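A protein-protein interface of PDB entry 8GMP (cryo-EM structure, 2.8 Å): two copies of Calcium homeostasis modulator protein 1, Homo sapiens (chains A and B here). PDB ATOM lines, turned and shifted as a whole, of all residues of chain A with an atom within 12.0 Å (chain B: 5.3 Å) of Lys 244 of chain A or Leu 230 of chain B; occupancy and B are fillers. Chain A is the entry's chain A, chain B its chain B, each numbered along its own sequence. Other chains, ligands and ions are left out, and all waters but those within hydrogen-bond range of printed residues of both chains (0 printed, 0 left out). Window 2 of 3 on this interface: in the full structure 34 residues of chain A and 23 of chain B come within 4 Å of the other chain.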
ATOM      1  N   CYS A 235     -10.476  -9.104 -14.364  1.00  0.00           N
ATOM      2  CA  CYS A 235      -9.673 -10.306 -14.193  1.00  0.00           C
ATOM      3  C   CYS A 235      -8.640 -10.488 -15.296  1.00  0.00           C
ATOM      4  O   CYS A 235      -7.672 -11.231 -15.096  1.00  0.00           O
ATOM      5  CB  CYS A 235     -10.573 -11.547 -14.138  1.00  0.00           C
ATOM      6  SG  CYS A 235     -11.439 -11.794 -12.572  1.00  0.00           S
ATOM      7  N   THR A 236      -8.820  -9.839 -16.447  1.00  0.00           N
ATOM      8  CA  THR A 236      -7.884  -9.981 -17.554  1.00  0.00           C
ATOM      9  C   THR A 236      -6.922  -8.804 -17.617  1.00  0.00           C
ATOM     10  O   THR A 236      -6.266  -8.590 -18.640  1.00  0.00           O
ATOM     11  CB  THR A 236      -8.642 -10.115 -18.887  1.00  0.00           C
ATOM     12  OG1 THR A 236      -9.460  -8.959 -19.094  1.00  0.00           O
ATOM     13  CG2 THR A 236      -9.652 -11.251 -18.815  1.00  0.00           C
ATOM     14  N   GLU A 237      -6.827  -8.036 -16.536  1.00  0.00           N
ATOM     15  CA  GLU A 237      -5.856  -6.952 -16.475  1.00  0.00           C
ATOM     16  C   GLU A 237      -5.005  -7.071 -15.221  1.00  0.00           C
ATOM     17  O   GLU A 237      -3.820  -6.726 -15.237  1.00  0.00           O
ATOM     18  CB  GLU A 237      -6.555  -5.593 -16.538  1.00  0.00           C
ATOM     19  CG  GLU A 237      -7.143  -5.277 -17.901  1.00  0.00           C
ATOM     20  CD  GLU A 237      -7.817  -3.925 -17.940  1.00  0.00           C
ATOM     21  OE1 GLU A 237      -7.942  -3.296 -16.868  1.00  0.00           O
ATOM     22  OE2 GLU A 237      -8.213  -3.487 -19.041  1.00  0.00           O
ATOM     23  N   HIS A 238      -5.597  -7.555 -14.130  1.00  0.00           N
ATOM     24  CA  HIS A 238      -4.807  -7.881 -12.952  1.00  0.00           C
ATOM     25  C   HIS A 238      -3.959  -9.126 -13.168  1.00  0.00           C
ATOM     26  O   HIS A 238      -2.971  -9.322 -12.454  1.00  0.00           O
ATOM     27  CB  HIS A 238      -5.722  -8.060 -11.737  1.00  0.00           C
ATOM     28  CG  HIS A 238      -4.992  -8.140 -10.432  1.00  0.00           C
ATOM     29  ND1 HIS A 238      -4.186  -9.207 -10.092  1.00  0.00           N
ATOM     30  CD2 HIS A 238      -4.936  -7.281  -9.389  1.00  0.00           C
ATOM     31  CE1 HIS A 238      -3.673  -9.004  -8.892  1.00  0.00           C
ATOM     32  NE2 HIS A 238      -4.113  -7.841  -8.443  1.00  0.00           N
ATOM     33  N   ALA A 239      -4.322  -9.968 -14.138  1.00  0.00           N
ATOM     34  CA  ALA A 239      -3.510 -11.136 -14.460  1.00  0.00           C
ATOM     35  C   ALA A 239      -2.453 -10.801 -15.505  1.00  0.00           C
ATOM     36  O   ALA A 239      -1.349 -11.353 -15.481  1.00  0.00           O
ATOM     37  CB  ALA A 239      -4.404 -12.277 -14.947  1.00  0.00           C
ATOM     38  N   LYS A 240      -2.776  -9.891 -16.429  1.00  0.00           N
ATOM     39  CA  LYS A 240      -1.853  -9.534 -17.500  1.00  0.00           C
ATOM     40  C   LYS A 240      -0.603  -8.823 -16.997  1.00  0.00           C
ATOM     41  O   LYS A 240       0.375  -8.723 -17.745  1.00  0.00           O
ATOM     42  CB  LYS A 240      -2.573  -8.662 -18.530  1.00  0.00           C
ATOM     43  CG  LYS A 240      -1.764  -8.387 -19.779  1.00  0.00           C
ATOM     44  CD  LYS A 240      -2.600  -7.689 -20.830  1.00  0.00           C
ATOM     45  CE  LYS A 240      -3.603  -8.647 -21.450  1.00  0.00           C
ATOM     46  NZ  LYS A 240      -4.323  -8.033 -22.597  1.00  0.00           N
ATOM     47  N   ALA A 241      -0.602  -8.336 -15.760  1.00  0.00           N
ATOM     48  CA  ALA A 241       0.598  -7.760 -15.173  1.00  0.00           C
ATOM     49  C   ALA A 241       1.513  -8.810 -14.559  1.00  0.00           C
ATOM     50  O   ALA A 241       2.706  -8.545 -14.386  1.00  0.00           O
ATOM     51  CB  ALA A 241       0.220  -6.721 -14.128  1.00  0.00           C
ATOM     52  N   PHE A 242       0.982  -9.985 -14.228  1.00  0.00           N
ATOM     53  CA  PHE A 242       1.782 -11.111 -13.764  1.00  0.00           C
ATOM     54  C   PHE A 242       2.259 -11.992 -14.909  1.00  0.00           C
ATOM     55  O   PHE A 242       3.231 -12.736 -14.753  1.00  0.00           O
ATOM     56  CB  PHE A 242       0.979 -11.956 -12.771  1.00  0.00           C
ATOM     57  CG  PHE A 242       0.937 -11.385 -11.381  1.00  0.00           C
ATOM     58  CD1 PHE A 242       2.041 -11.469 -10.550  1.00  0.00           C
ATOM     59  CD2 PHE A 242      -0.204 -10.761 -10.910  1.00  0.00           C
ATOM     60  CE1 PHE A 242       2.006 -10.945  -9.273  1.00  0.00           C
ATOM     61  CE2 PHE A 242      -0.245 -10.233  -9.633  1.00  0.00           C
ATOM     62  CZ  PHE A 242       0.861 -10.326  -8.815  1.00  0.00           C
ATOM     63  N   ALA A 243       1.584 -11.926 -16.057  1.00  0.00           N
ATOM     64  CA  ALA A 243       2.013 -12.690 -17.223  1.00  0.00           C
ATOM     65  C   ALA A 243       3.377 -12.221 -17.716  1.00  0.00           C
ATOM     66  O   ALA A 243       4.288 -13.031 -17.923  1.00  0.00           O
ATOM     67  CB  ALA A 243       0.967 -12.582 -18.331  1.00  0.00           C
ATOM     68  N   LYS A 244       3.536 -10.907 -17.907  1.00  0.00           N
ATOM     69  CA  LYS A 244       4.797 -10.347 -18.386  1.00  0.00           C
ATOM     70  C   LYS A 244       5.981 -10.673 -17.485  1.00  0.00           C
ATOM     71  O   LYS A 244       7.106 -10.763 -17.986  1.00  0.00           O
ATOM     72  CB  LYS A 244       4.688  -8.828 -18.535  1.00  0.00           C
ATOM     73  CG  LYS A 244       3.740  -8.355 -19.623  1.00  0.00           C
ATOM     74  CD  LYS A 244       3.793  -6.840 -19.764  1.00  0.00           C
ATOM     75  CE  LYS A 244       2.428  -6.207 -19.588  1.00  0.00           C
ATOM     76  NZ  LYS A 244       1.503  -6.566 -20.692  1.00  0.00           N
ATOM     77  N   VAL A 245       5.772 -10.843 -16.178  1.00  0.00           N
ATOM     78  CA  VAL A 245       6.865 -11.224 -15.290  1.00  0.00           C
ATOM     79  C   VAL A 245       7.111 -12.727 -15.293  1.00  0.00           C
ATOM     80  O   VAL A 245       8.201 -13.166 -14.892  1.00  0.00           O
ATOM     81  CB  VAL A 245       6.622 -10.734 -13.844  1.00  0.00           C
ATOM     82  CG1 VAL A 245       5.442 -11.452 -13.216  1.00  0.00           C
ATOM     83  CG2 VAL A 245       7.879 -10.912 -13.001  1.00  0.00           C
ATOM     84  N   CYS A 246       6.148 -13.528 -15.751  1.00  0.00           N
ATOM     85  CA  CYS A 246       6.350 -14.971 -15.829  1.00  0.00           C
ATOM     86  C   CYS A 246       7.037 -15.363 -17.131  1.00  0.00           C
ATOM     87  O   CYS A 246       7.923 -16.225 -17.139  1.00  0.00           O
ATOM     88  CB  CYS A 246       5.010 -15.695 -15.687  1.00  0.00           C
ATOM     89  SG  CYS A 246       5.108 -17.491 -15.854  1.00  0.00           S
ATOM     90  N   ILE A 247       6.642 -14.737 -18.242  1.00  0.00           N
ATOM     91  CA  ILE A 247       7.214 -15.063 -19.542  1.00  0.00           C
ATOM     92  C   ILE A 247       8.700 -14.757 -19.608  1.00  0.00           C
ATOM     93  O   ILE A 247       9.490 -15.621 -19.999  1.00  0.00           O
ATOM     94  CB  ILE A 247       6.456 -14.314 -20.655  1.00  0.00           C
ATOM     95  CG1 ILE A 247       5.195 -15.081 -21.052  1.00  0.00           C
ATOM     96  CG2 ILE A 247       7.355 -14.093 -21.851  1.00  0.00           C
ATOM     97  CD1 ILE A 247       4.344 -14.359 -22.063  1.00  0.00           C
ATOM     98  N   GLN A 248       9.111 -13.549 -19.222  1.00  0.00           N
ATOM     99  CA  GLN A 248      10.532 -13.218 -19.255  1.00  0.00           C
ATOM    100  C   GLN A 248      11.328 -14.001 -18.219  1.00  0.00           C
ATOM    101  O   GLN A 248      12.550 -14.124 -18.349  1.00  0.00           O
ATOM    102  CB  GLN A 248      10.726 -11.715 -19.060  1.00  0.00           C
ATOM    103  CG  GLN A 248      10.298 -10.883 -20.255  1.00  0.00           C
ATOM    104  CD  GLN A 248      10.138  -9.417 -19.911  1.00  0.00           C
ATOM    105  OE1 GLN A 248       9.156  -9.018 -19.287  1.00  0.00           O
ATOM    106  NE2 GLN A 248      11.115  -8.607 -20.300  1.00  0.00           N
ATOM    107  N   GLN A 249      10.665 -14.536 -17.198  1.00  0.00           N
ATOM    108  CA  GLN A 249      11.295 -15.460 -16.268  1.00  0.00           C
ATOM    109  C   GLN A 249      11.385 -16.868 -16.842  1.00  0.00           C
ATOM    110  O   GLN A 249      12.245 -17.647 -16.419  1.00  0.00           O
ATOM    111  CB  GLN A 249      10.530 -15.465 -14.940  1.00  0.00           C
ATOM    112  CG  GLN A 249      11.239 -16.162 -13.790  1.00  0.00           C
ATOM    113  CD  GLN A 249      10.925 -17.639 -13.715  1.00  0.00           C
ATOM    114  OE1 GLN A 249       9.842 -18.076 -14.105  1.00  0.00           O
ATOM    115  NE2 GLN A 249      11.873 -18.420 -13.216  1.00  0.00           N
ATOM    116  N   PHE A 250      10.524 -17.202 -17.805  1.00  0.00           N
ATOM    117  CA  PHE A 250      10.630 -18.442 -18.562  1.00  0.00           C
ATOM    118  C   PHE A 250      11.286 -18.255 -19.918  1.00  0.00           C
ATOM    119  O   PHE A 250      11.634 -19.255 -20.556  1.00  0.00           O
ATOM    120  CB  PHE A 250       9.247 -19.077 -18.764  1.00  0.00           C
ATOM    121  N   PHE A 251      11.459 -17.020 -20.377  1.00  0.00           N
ATOM    122  CA  PHE A 251      12.305 -16.716 -21.515  1.00  0.00           C
ATOM    123  C   PHE A 251      13.765 -16.604 -21.094  1.00  0.00           C
ATOM    124  O   PHE A 251      14.623 -16.308 -21.931  1.00  0.00           O
ATOM    125  CB  PHE A 251      11.829 -15.416 -22.178  1.00  0.00           C
ATOM    126  CG  PHE A 251      11.947 -15.415 -23.673  1.00  0.00           C
ATOM    127  CD1 PHE A 251      10.977 -16.032 -24.449  1.00  0.00           C
ATOM    128  CD2 PHE A 251      13.008 -14.796 -24.304  1.00  0.00           C
ATOM    129  CE1 PHE A 251      11.066 -16.036 -25.822  1.00  0.00           C
ATOM    130  CE2 PHE A 251      13.104 -14.800 -25.681  1.00  0.00           C
ATOM    131  CZ  PHE A 251      12.132 -15.420 -26.439  1.00  0.00           C
ATOM    132  N   GLU A 252      14.051 -16.836 -19.810  1.00  0.00           N
ATOM    133  CA  GLU A 252      15.394 -17.006 -19.275  1.00  0.00           C
ATOM    134  C   GLU A 252      16.015 -18.341 -19.636  1.00  0.00           C
ATOM    135  O   GLU A 252      17.247 -18.440 -19.684  1.00  0.00           O
ATOM    136  CB  GLU A 252      15.373 -16.844 -17.753  1.00  0.00           C
ATOM    137  N   ALA A 253      15.203 -19.363 -19.887  1.00  0.00           N
ATOM    138  CA  ALA A 253      15.718 -20.700 -20.088  1.00  0.00           C
ATOM    139  C   ALA A 253      16.093 -21.003 -21.521  1.00  0.00           C
ATOM    140  O   ALA A 253      17.186 -21.508 -21.789  1.00  0.00           O
ATOM    141  CB  ALA A 253      14.702 -21.720 -19.596  1.00  0.00           C
ATOM    142  N   MET A 254      15.190 -20.707 -22.449  1.00  0.00           N
ATOM    143  CA  MET A 254      15.374 -21.048 -23.853  1.00  0.00           C
ATOM    144  C   MET A 254      16.102 -19.971 -24.648  1.00  0.00           C
ATOM    145  O   MET A 254      15.986 -19.952 -25.879  1.00  0.00           O
ATOM    146  CB  MET A 254      14.015 -21.345 -24.489  1.00  0.00           C
ATOM    147  CG  MET A 254      12.952 -20.332 -24.138  1.00  0.00           C
ATOM    148  SD  MET A 254      11.325 -20.780 -24.758  1.00  0.00           S
ATOM    149  CE  MET A 254      10.325 -19.555 -23.925  1.00  0.00           C
ATOM    150  N   ASP B 225      -5.381 -18.155 -20.199  1.00  0.00           N
ATOM    151  CA  ASP B 225      -5.498 -17.729 -21.589  1.00  0.00           C
ATOM    152  C   ASP B 225      -4.603 -16.532 -21.888  1.00  0.00           C
ATOM    153  O   ASP B 225      -3.978 -16.466 -22.952  1.00  0.00           O
ATOM    154  CB  ASP B 225      -6.956 -17.411 -21.914  1.00  0.00           C
ATOM    155  CG  ASP B 225      -7.766 -18.653 -22.212  1.00  0.00           C
ATOM    156  OD1 ASP B 225      -7.869 -19.026 -23.401  1.00  0.00           O
ATOM    157  OD2 ASP B 225      -8.291 -19.266 -21.259  1.00  0.00           O
ATOM    158  N   ILE B 226      -4.531 -15.570 -20.966  1.00  0.00           N
ATOM    159  CA  ILE B 226      -3.769 -14.355 -21.241  1.00  0.00           C
ATOM    160  C   ILE B 226      -2.276 -14.650 -21.277  1.00  0.00           C
ATOM    161  O   ILE B 226      -1.533 -14.067 -22.074  1.00  0.00           O
ATOM    162  CB  ILE B 226      -4.110 -13.263 -20.213  1.00  0.00           C
ATOM    163  CG1 ILE B 226      -5.608 -12.963 -20.239  1.00  0.00           C
ATOM    164  CG2 ILE B 226      -3.319 -12.001 -20.504  1.00  0.00           C
ATOM    165  CD1 ILE B 226      -6.118 -12.492 -21.586  1.00  0.00           C
ATOM    166  N   GLU B 227      -1.808 -15.555 -20.417  1.00  0.00           N
ATOM    167  CA  GLU B 227      -0.407 -15.953 -20.465  1.00  0.00           C
ATOM    168  C   GLU B 227      -0.072 -16.701 -21.747  1.00  0.00           C
ATOM    169  O   GLU B 227       1.090 -16.708 -22.164  1.00  0.00           O
ATOM    170  CB  GLU B 227      -0.061 -16.819 -19.252  1.00  0.00           C
ATOM    171  CG  GLU B 227       1.350 -17.369 -19.275  1.00  0.00           C
ATOM    172  CD  GLU B 227       1.830 -17.795 -17.905  1.00  0.00           C
ATOM    173  OE1 GLU B 227       1.869 -16.940 -16.998  1.00  0.00           O
ATOM    174  OE2 GLU B 227       2.164 -18.985 -17.734  1.00  0.00           O
ATOM    175  N   ARG B 228      -1.064 -17.323 -22.383  1.00  0.00           N
ATOM    176  CA  ARG B 228      -0.835 -17.994 -23.656  1.00  0.00           C
ATOM    177  C   ARG B 228      -0.652 -16.986 -24.784  1.00  0.00           C
ATOM    178  O   ARG B 228       0.354 -17.021 -25.501  1.00  0.00           O
ATOM    179  CB  ARG B 228      -1.996 -18.941 -23.959  1.00  0.00           C
ATOM    180  CG  ARG B 228      -1.882 -19.672 -25.279  1.00  0.00           C
ATOM    181  CD  ARG B 228      -3.096 -20.553 -25.512  1.00  0.00           C
ATOM    182  NE  ARG B 228      -3.458 -21.310 -24.317  1.00  0.00           N
ATOM    183  CZ  ARG B 228      -2.836 -22.414 -23.916  1.00  0.00           C
ATOM    184  NH1 ARG B 228      -1.815 -22.891 -24.614  1.00  0.00           N
ATOM    185  NH2 ARG B 228      -3.232 -23.041 -22.816  1.00  0.00           N
ATOM    186  N   LYS B 229      -1.617 -16.077 -24.954  1.00  0.00           N
ATOM    187  CA  LYS B 229      -1.542 -15.101 -26.033  1.00  0.00           C
ATOM    188  C   LYS B 229      -0.377 -14.134 -25.868  1.00  0.00           C
ATOM    189  O   LYS B 229       0.096 -13.581 -26.866  1.00  0.00           O
ATOM    190  CB  LYS B 229      -2.851 -14.318 -26.125  1.00  0.00           C
ATOM    191  CG  LYS B 229      -4.053 -15.161 -26.522  1.00  0.00           C
ATOM    192  CD  LYS B 229      -5.314 -14.316 -26.593  1.00  0.00           C
ATOM    193  CE  LYS B 229      -6.503 -15.135 -27.061  1.00  0.00           C
ATOM    194  NZ  LYS B 229      -6.879 -16.178 -26.070  1.00  0.00           N
ATOM    195  N   LEU B 230       0.092 -13.911 -24.639  1.00  0.00           N
ATOM    196  CA  LEU B 230       1.265 -13.066 -24.449  1.00  0.00           C
ATOM    197  C   LEU B 230       2.548 -13.786 -24.836  1.00  0.00           C
ATOM    198  O   LEU B 230       3.502 -13.146 -25.287  1.00  0.00           O
ATOM    199  CB  LEU B 230       1.351 -12.596 -22.997  1.00  0.00           C
ATOM    200  CG  LEU B 230       0.661 -11.278 -22.641  1.00  0.00           C
ATOM    201  CD1 LEU B 230       1.089 -10.812 -21.259  1.00  0.00           C
ATOM    202  CD2 LEU B 230       0.954 -10.211 -23.682  1.00  0.00           C
ATOM    203  N   PHE B 231       2.588 -15.108 -24.668  1.00  0.00           N
ATOM    204  CA  PHE B 231       3.792 -15.866 -24.993  1.00  0.00           C
ATOM    205  C   PHE B 231       4.025 -15.912 -26.498  1.00  0.00           C
ATOM    206  O   PHE B 231       5.162 -15.787 -26.965  1.00  0.00           O
ATOM    207  CB  PHE B 231       3.691 -17.279 -24.419  1.00  0.00           C
ATOM    208  CG  PHE B 231       4.868 -18.149 -24.744  1.00  0.00           C
ATOM    209  CD1 PHE B 231       6.088 -17.941 -24.127  1.00  0.00           C
ATOM    210  CD2 PHE B 231       4.756 -19.173 -25.667  1.00  0.00           C
ATOM    211  CE1 PHE B 231       7.171 -18.737 -24.425  1.00  0.00           C
ATOM    212  CE2 PHE B 231       5.839 -19.974 -25.967  1.00  0.00           C
ATOM    213  CZ  PHE B 231       7.048 -19.756 -25.345  1.00  0.00           C
ATOM    214  N   ASP B 232       2.955 -16.102 -27.273  1.00  0.00           N
ATOM    215  CA  ASP B 232       3.095 -16.244 -28.719  1.00  0.00           C
ATOM    216  C   ASP B 232       3.658 -14.984 -29.360  1.00  0.00           C
ATOM    217  O   ASP B 232       4.608 -15.049 -30.149  1.00  0.00           O
ATOM    218  CB  ASP B 232       1.745 -16.590 -29.342  1.00  0.00           C
ATOM    219  CG  ASP B 232       1.224 -17.927 -28.881  1.00  0.00           C
ATOM    220  OD1 ASP B 232       2.036 -18.737 -28.390  1.00  0.00           O
ATOM    221  OD2 ASP B 232       0.008 -18.171 -29.012  1.00  0.00           O
ATOM    222  N   GLU B 233       3.086 -13.824 -29.036  1.00  0.00           N
ATOM    223  CA  GLU B 233       3.512 -12.594 -29.694  1.00  0.00           C
ATOM    224  C   GLU B 233       4.895 -12.160 -29.224  1.00  0.00           C
ATOM    225  O   GLU B 233       5.545 -11.331 -29.872  1.00  0.00           O
ATOM    226  CB  GLU B 233       2.479 -11.495 -29.469  1.00  0.00           C
ATOM    227  CG  GLU B 233       1.192 -11.743 -30.231  1.00  0.00           C
ATOM    228  CD  GLU B 233       0.164 -10.658 -30.010  1.00  0.00           C
ATOM    229  OE1 GLU B 233       0.393  -9.788 -29.144  1.00  0.00           O
ATOM    230  OE2 GLU B 233      -0.873 -10.669 -30.705  1.00  0.00           O
ATOM    231  N   THR B 234       5.366 -12.708 -28.104  1.00  0.00           N
ATOM    232  CA  THR B 234       6.755 -12.523 -27.716  1.00  0.00           C
ATOM    233  C   THR B 234       7.686 -13.492 -28.431  1.00  0.00           C
ATOM    234  O   THR B 234       8.898 -13.261 -28.457  1.00  0.00           O
ATOM    235  CB  THR B 234       6.911 -12.689 -26.203  1.00  0.00           C
ATOM    236  OG1 THR B 234       5.910 -11.918 -25.526  1.00  0.00           O
ATOM    237  CG2 THR B 234       8.288 -12.219 -25.756  1.00  0.00           C
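Of the 10 printed residues of chain B, 4 touch a printed residue of chain A. Printed residues of chain B that touch a printed residue of chain A: Ile 226, Glu 227, Leu 230 and Phe 231. Hydrophobic or aromatic side chains of chain B that line the printed part of chain A: Ile 226, Leu 230 and Phe 231.
O of Lys 244 of chain A sits close to OE1 of Gln 248 of chain A (3.0 Å). The backbone carbonyl oxygen (O) of Leu 230 of chain B is in hydrogen-bond range of the side-chain hydroxyl (OG1) of Thr 234 of chain B, at 2.7 Å.
SG of Cys 246 of chain A sits at hydrogen-bond distance from OE1 of Glu 227 of chain B (3.5 Å).
Printed residues of chain B within 4 Å of Lys 240 of chain A: Ile 226 (3.5 Å). Printed residues of chain B within 4 Å of Ala 243 of chain A: Leu 230. Of chain B, only Leu 230 comes within 4 Å of Lys 244 of chain A. Printed residues of chain B within 4 Å of Cys 246 of chain A: Glu 227 (3.5 Å). Of the printed residues of chain B, Met 254 of chain A touches Phe 231 (3.3 Å). Ile 226 of chain B touches just one residue of chain A: Lys 240. Printed residues of chain A within 4 Å of Glu 227 of chain B: Cys 246 (3.5 Å). Leu 230 of chain B touches three residues of chain A. Phe 231 of chain B touches just these residues of chain A: Ile 247 and Met 254. The nearest printed residue of chain B that does not touch Lys 244 of chain A is Glu 227 of chain B (6.3 Å). The nearest printed residue of chain B that does not touch Met 254 of chain A is Thr 234 of chain B (7.8 Å).
CE of Lys 240 of chain A touches CG2 of Ile 226 of chain B (3.5 Å). Leu 230 of chain B touches Ala 243 of chain A (CD1 to CB, 3.4 Å). Lys 244 of chain A touches Leu 230 of chain B. C of Leu 230 of chain B touches CD1 of Ile 247 of chain A, at 3.4 Å. Ile 247 of chain A touches Phe 231 of chain B. Phe 231 of chain B touches Met 254 of chain A.
No position is printed for both chains. Of the 7 pairs that touch across the chains among the printed residues, none has its exchanged pair printed and touching as well.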
